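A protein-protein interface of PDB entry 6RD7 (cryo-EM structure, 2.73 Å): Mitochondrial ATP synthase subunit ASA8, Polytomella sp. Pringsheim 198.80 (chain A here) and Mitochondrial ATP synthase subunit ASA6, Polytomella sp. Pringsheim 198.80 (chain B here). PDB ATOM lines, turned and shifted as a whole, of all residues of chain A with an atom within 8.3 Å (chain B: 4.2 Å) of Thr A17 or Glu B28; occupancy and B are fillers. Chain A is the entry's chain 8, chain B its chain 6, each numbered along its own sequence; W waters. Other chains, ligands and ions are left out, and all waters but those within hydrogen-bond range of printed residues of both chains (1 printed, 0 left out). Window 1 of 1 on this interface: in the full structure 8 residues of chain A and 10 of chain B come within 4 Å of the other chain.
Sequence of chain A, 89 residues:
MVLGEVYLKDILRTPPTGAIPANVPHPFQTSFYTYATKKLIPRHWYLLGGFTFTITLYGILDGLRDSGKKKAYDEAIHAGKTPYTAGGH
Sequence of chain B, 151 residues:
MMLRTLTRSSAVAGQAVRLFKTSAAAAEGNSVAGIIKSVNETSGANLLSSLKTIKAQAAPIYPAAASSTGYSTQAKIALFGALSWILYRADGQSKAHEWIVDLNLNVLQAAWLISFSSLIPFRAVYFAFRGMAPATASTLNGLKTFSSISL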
ATOM      1  N   GLU A   5      -4.559  11.762 -12.299  1.00  0.00           N
ATOM      2  CA  GLU A   5      -4.077  10.826 -13.312  1.00  0.00           C
ATOM      3  C   GLU A   5      -2.960   9.948 -12.770  1.00  0.00           C
ATOM      4  O   GLU A   5      -2.811   8.793 -13.185  1.00  0.00           O
ATOM      5  CB  GLU A   5      -3.581  11.593 -14.536  1.00  0.00           C
ATOM      6  CG  GLU A   5      -4.654  12.030 -15.502  1.00  0.00           C
ATOM      7  CD  GLU A   5      -4.133  12.152 -16.922  1.00  0.00           C
ATOM      8  OE1 GLU A   5      -4.383  13.193 -17.564  1.00  0.00           O
ATOM      9  OE2 GLU A   5      -3.473  11.204 -17.396  1.00  0.00           O
ATOM     10  N   LYS A   9      -1.743   5.857 -13.481  1.00  0.00           N
ATOM     11  CA  LYS A   9      -0.838   6.240 -14.562  1.00  0.00           C
ATOM     12  C   LYS A   9      -0.545   5.074 -15.498  1.00  0.00           C
ATOM     13  O   LYS A   9      -0.724   5.182 -16.716  1.00  0.00           O
ATOM     14  CB  LYS A   9       0.460   6.790 -13.976  1.00  0.00           C
ATOM     15  CG  LYS A   9       1.540   7.023 -15.008  1.00  0.00           C
ATOM     16  CD  LYS A   9       2.851   7.427 -14.359  1.00  0.00           C
ATOM     17  CE  LYS A   9       3.472   6.269 -13.600  1.00  0.00           C
ATOM     18  NZ  LYS A   9       4.432   5.498 -14.437  1.00  0.00           N
ATOM     19  N   LEU A  12      -4.661   1.865 -15.238  1.00  0.00           N
ATOM     20  CA  LEU A  12      -5.889   1.925 -16.015  1.00  0.00           C
ATOM     21  C   LEU A  12      -5.786   3.041 -17.036  1.00  0.00           C
ATOM     22  O   LEU A  12      -5.447   4.176 -16.693  1.00  0.00           O
ATOM     23  CB  LEU A  12      -7.103   2.174 -15.128  1.00  0.00           C
ATOM     24  CG  LEU A  12      -7.531   1.046 -14.199  1.00  0.00           C
ATOM     25  CD1 LEU A  12      -8.523   1.577 -13.199  1.00  0.00           C
ATOM     26  CD2 LEU A  12      -8.125  -0.092 -14.997  1.00  0.00           C
ATOM     27  N   ARG A  13      -6.071   2.719 -18.292  1.00  0.00           N
ATOM     28  CA  ARG A  13      -6.115   3.712 -19.350  1.00  0.00           C
ATOM     29  C   ARG A  13      -7.456   3.626 -20.059  1.00  0.00           C
ATOM     30  O   ARG A  13      -8.091   2.572 -20.112  1.00  0.00           O
ATOM     31  CB  ARG A  13      -4.970   3.527 -20.353  1.00  0.00           C
ATOM     32  CG  ARG A  13      -3.610   3.370 -19.716  1.00  0.00           C
ATOM     33  CD  ARG A  13      -2.503   3.680 -20.677  1.00  0.00           C
ATOM     34  NE  ARG A  13      -1.207   3.311 -20.126  1.00  0.00           N
ATOM     35  CZ  ARG A  13      -0.607   2.153 -20.356  1.00  0.00           C
ATOM     36  NH1 ARG A  13       0.570   1.896 -19.812  1.00  0.00           N
ATOM     37  NH2 ARG A  13      -1.186   1.251 -21.129  1.00  0.00           N
ATOM     38  N   THR A  14      -7.880   4.746 -20.587  1.00  0.00           N
ATOM     39  CA  THR A  14      -9.079   4.900 -21.391  1.00  0.00           C
ATOM     40  C   THR A  14      -8.797   4.432 -22.814  1.00  0.00           C
ATOM     41  O   THR A  14      -7.643   4.150 -23.148  1.00  0.00           O
ATOM     42  CB  THR A  14      -9.514   6.365 -21.368  1.00  0.00           C
ATOM     43  OG1 THR A  14      -8.416   7.185 -21.765  1.00  0.00           O
ATOM     44  CG2 THR A  14      -9.977   6.751 -19.983  1.00  0.00           C
ATOM     45  N   PRO A  15      -9.817   4.274 -23.666  1.00  0.00           N
ATOM     46  CA  PRO A  15      -9.550   4.004 -25.088  1.00  0.00           C
ATOM     47  C   PRO A  15      -8.761   5.131 -25.726  1.00  0.00           C
ATOM     48  O   PRO A  15      -8.971   6.306 -25.393  1.00  0.00           O
ATOM     49  CB  PRO A  15     -10.953   3.892 -25.701  1.00  0.00           C
ATOM     50  CG  PRO A  15     -11.894   4.329 -24.638  1.00  0.00           C
ATOM     51  CD  PRO A  15     -11.232   3.991 -23.365  1.00  0.00           C
ATOM     52  N   PRO A  16      -7.819   4.804 -26.612  1.00  0.00           N
ATOM     53  CA  PRO A  16      -6.916   5.828 -27.148  1.00  0.00           C
ATOM     54  C   PRO A  16      -7.646   6.807 -28.050  1.00  0.00           C
ATOM     55  O   PRO A  16      -8.575   6.443 -28.769  1.00  0.00           O
ATOM     56  CB  PRO A  16      -5.879   5.011 -27.922  1.00  0.00           C
ATOM     57  CG  PRO A  16      -6.562   3.741 -28.236  1.00  0.00           C
ATOM     58  CD  PRO A  16      -7.458   3.460 -27.084  1.00  0.00           C
ATOM     59  N   THR A  17      -7.233   8.069 -27.975  1.00  0.00           N
ATOM     60  CA  THR A  17      -7.885   9.159 -28.688  1.00  0.00           C
ATOM     61  C   THR A  17      -7.010   9.739 -29.789  1.00  0.00           C
ATOM     62  O   THR A  17      -7.524  10.299 -30.759  1.00  0.00           O
ATOM     63  CB  THR A  17      -8.278  10.265 -27.704  1.00  0.00           C
ATOM     64  OG1 THR A  17      -7.166  10.561 -26.853  1.00  0.00           O
ATOM     65  CG2 THR A  17      -9.447   9.826 -26.850  1.00  0.00           C
ATOM     66  N   GLY A  18      -5.690   9.626 -29.650  1.00  0.00           N
ATOM     67  CA  GLY A  18      -4.808  10.174 -30.665  1.00  0.00           C
ATOM     68  C   GLY A  18      -4.481   9.172 -31.753  1.00  0.00           C
ATOM     69  O   GLY A  18      -4.692   9.431 -32.941  1.00  0.00           O
ATOM     70  N   ALA A  19      -3.962   8.013 -31.364  1.00  0.00           N
ATOM     71  CA  ALA A  19      -3.569   6.991 -32.320  1.00  0.00           C
ATOM     72  C   ALA A  19      -3.643   5.635 -31.645  1.00  0.00           C
ATOM     73  O   ALA A  19      -3.491   5.518 -30.426  1.00  0.00           O
ATOM     74  CB  ALA A  19      -2.161   7.240 -32.866  1.00  0.00           C
ATOM     75  N   ILE A  20      -3.881   4.613 -32.451  1.00  0.00           N
ATOM     76  CA  ILE A  20      -3.895   3.239 -31.950  1.00  0.00           C
ATOM     77  C   ILE A  20      -2.458   2.807 -31.679  1.00  0.00           C
ATOM     78  O   ILE A  20      -1.609   2.927 -32.574  1.00  0.00           O
ATOM     79  CB  ILE A  20      -4.572   2.313 -32.954  1.00  0.00           C
ATOM     80  CG1 ILE A  20      -6.072   2.589 -32.987  1.00  0.00           C
ATOM     81  CG2 ILE A  20      -4.312   0.855 -32.612  1.00  0.00           C
ATOM     82  CD1 ILE A  20      -6.830   1.666 -33.879  1.00  0.00           C
ATOM     83  N   PRO A  21      -2.143   2.324 -30.481  1.00  0.00           N
ATOM     84  CA  PRO A  21      -0.758   1.975 -30.164  1.00  0.00           C
ATOM     85  C   PRO A  21      -0.322   0.697 -30.859  1.00  0.00           C
ATOM     86  O   PRO A  21      -1.103   0.005 -31.511  1.00  0.00           O
ATOM     87  CB  PRO A  21      -0.777   1.783 -28.641  1.00  0.00           C
ATOM     88  CG  PRO A  21      -2.127   2.237 -28.190  1.00  0.00           C
ATOM     89  CD  PRO A  21      -3.036   2.071 -29.343  1.00  0.00           C
ATOM     90  N   GLU B  28      -1.155   8.712 -24.617  1.00  0.00           N
ATOM     91  CA  GLU B  28      -1.551  10.055 -24.213  1.00  0.00           C
ATOM     92  C   GLU B  28      -2.252  10.022 -22.861  1.00  0.00           C
ATOM     93  O   GLU B  28      -2.400   8.956 -22.261  1.00  0.00           O
ATOM     94  CB  GLU B  28      -2.460  10.684 -25.271  1.00  0.00           C
ATOM     95  CG  GLU B  28      -3.840  10.054 -25.370  1.00  0.00           C
ATOM     96  CD  GLU B  28      -3.919   8.940 -26.398  1.00  0.00           C
ATOM     97  OE1 GLU B  28      -2.862   8.449 -26.842  1.00  0.00           O
ATOM     98  OE2 GLU B  28      -5.049   8.558 -26.765  1.00  0.00           O
ATOM     99  N   GLY B  29      -2.667  11.191 -22.379  1.00  0.00           N
ATOM    100  CA  GLY B  29      -3.439  11.245 -21.154  1.00  0.00           C
ATOM    101  C   GLY B  29      -4.827  10.669 -21.347  1.00  0.00           C
ATOM    102  O   GLY B  29      -5.332  10.565 -22.463  1.00  0.00           O
ATOM    103  N   ASN B  30      -5.456  10.288 -20.242  1.00  0.00           N
ATOM    104  CA  ASN B  30      -6.711   9.569 -20.362  1.00  0.00           C
ATOM    105  C   ASN B  30      -7.876  10.526 -20.597  1.00  0.00           C
ATOM    106  O   ASN B  30      -7.820  11.708 -20.257  1.00  0.00           O
ATOM    107  CB  ASN B  30      -6.955   8.691 -19.135  1.00  0.00           C
ATOM    108  CG  ASN B  30      -7.366   9.470 -17.933  1.00  0.00           C
ATOM    109  OD1 ASN B  30      -6.682  10.397 -17.531  1.00  0.00           O
ATOM    110  ND2 ASN B  30      -8.479   9.086 -17.329  1.00  0.00           N
ATOM    111  N   GLN B  57     -13.903  15.202 -28.191  1.00  0.00           N
ATOM    112  CA  GLN B  57     -12.494  15.121 -27.832  1.00  0.00           C
ATOM    113  C   GLN B  57     -12.236  13.933 -26.919  1.00  0.00           C
ATOM    114  O   GLN B  57     -11.082  13.590 -26.643  1.00  0.00           O
ATOM    115  CB  GLN B  57     -12.039  16.422 -27.180  1.00  0.00           C
ATOM    116  CG  GLN B  57     -12.189  17.628 -28.084  1.00  0.00           C
ATOM    117  CD  GLN B  57     -11.896  18.929 -27.373  1.00  0.00           C
ATOM    118  OE1 GLN B  57     -12.574  19.291 -26.412  1.00  0.00           O
ATOM    119  NE2 GLN B  57     -10.883  19.645 -27.844  1.00  0.00           N
ATOM    120  N   ALA B  58     -13.301  13.287 -26.447  1.00  0.00           N
ATOM    121  CA  ALA B  58     -13.121  12.109 -25.612  1.00  0.00           C
ATOM    122  C   ALA B  58     -13.477  10.836 -26.352  1.00  0.00           C
ATOM    123  O   ALA B  58     -13.317   9.742 -25.802  1.00  0.00           O
ATOM    124  CB  ALA B  58     -13.967  12.221 -24.354  1.00  0.00           C
ATOM    125  N   ALA B  59     -13.987  10.965 -27.568  1.00  0.00           N
ATOM    126  CA  ALA B  59     -14.304   9.803 -28.375  1.00  0.00           C
ATOM    127  C   ALA B  59     -13.015   9.089 -28.767  1.00  0.00           C
ATOM    128  O   ALA B  59     -11.993   9.747 -28.997  1.00  0.00           O
ATOM    129  CB  ALA B  59     -15.081  10.226 -29.623  1.00  0.00           C
ATOM    130  N   ILE B  61     -10.180   7.128 -30.986  1.00  0.00           N
ATOM    131  CA  ILE B  61      -9.772   7.273 -32.379  1.00  0.00           C
ATOM    132  C   ILE B  61     -10.179   5.991 -33.099  1.00  0.00           C
ATOM    133  O   ILE B  61      -9.847   4.877 -32.689  1.00  0.00           O
ATOM    134  CB  ILE B  61      -8.279   7.591 -32.537  1.00  0.00           C
ATOM    135  CG1 ILE B  61      -7.902   7.660 -34.015  1.00  0.00           C
ATOM    136  CG2 ILE B  61      -7.359   6.629 -31.792  1.00  0.00           C
ATOM    137  CD1 ILE B  61      -8.545   8.807 -34.746  1.00  0.00           C
HETATM  138  O   HOH W   1     -11.575   7.652 -25.021  1.00  0.00           O
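The backbone NH (N) of Thr A17 lies within hydrogen-bond range of the side-chain carboxylate (OE2) of Glu B28 (2.5 Å).
The side-chain carboxylate (OE2) of Glu B28 is in hydrogen-bond range of the backbone NH (N) of Gly A18, 3.1 Å away.
The side-chain amide oxygen (OD1) of Asn B30 sits close to the side-chain carboxylate (OE2) of Glu A5.
O of Pro A16 sits at hydrogen-bond distance from N of Ile B61.
Arg A13 touches none of the printed residues of chain B.
Of the printed residues of chain B, Thr A14 touches Asn B30.
Of chain A, only Pro A16, Thr A17 and Gly A18 come within 4 Å of Glu B28.
Printed residues of chain A within 4 Å of Gly B29: Glu A5 (3.8 Å).
Of the printed residues of chain A, Asn B30 touches Glu A5 and Thr A14.
Printed residues of chain A within 4 Å of Ile B61: Pro A16, Thr A17, Gly A18 and Ala A19.
The nearest residue of chain A that does not touch Glu B28 is Ala A19 (4.7 Å).
The nearest printed residue of chain B that does not touch Glu A5 is Glu B28 (5.5 Å).
OE2 of Glu A5 touches CA of Gly B29 (3.8 Å).
Thr A14 touches Asn B30.
OE2 of Glu B28 touches CA of Pro A16, 3.3 Å away.
CG2 of Thr A17 touches O of Ala B59, 3.3 Å away.
CB of Ile B61 touches O of Thr A17, 3.3 Å away.
Ile B61 touches Gly A18 (CG1 to O, 3.8 Å).
Ile B61 touches Ala A19 (CG2 to N, 3.7 Å).
Water W1 lies within hydrogen-bond range of the backbone carbonyl oxygen of Ala B58 (2.8 Å) and the backbone carbonyl oxygen of Pro A15 (3.0 Å).
Printed residues of chain B that touch a printed residue of chain A: Glu B28, Gly B29, Asn B30, Ala B59 and Ile B61.
Hydrophobic or aromatic side chains of chain B that line the printed part of chain A: Ile B61.
Of the 12 printed residues of chain A, 6 touch a printed residue of chain B.
Printed residues of chain A that touch a printed residue of chain B: Glu A5, Thr A14, Pro A16, Thr A17, Gly A18 and Ala A19.
Hydrophobic or aromatic side chains of chain A within 4 Å of the printed part of chain B: Pro A16.
Among the printed residues, no Asp or Glu carboxylate lies within 4 Å of a Lys or Arg side-chain nitrogen of the other chain.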
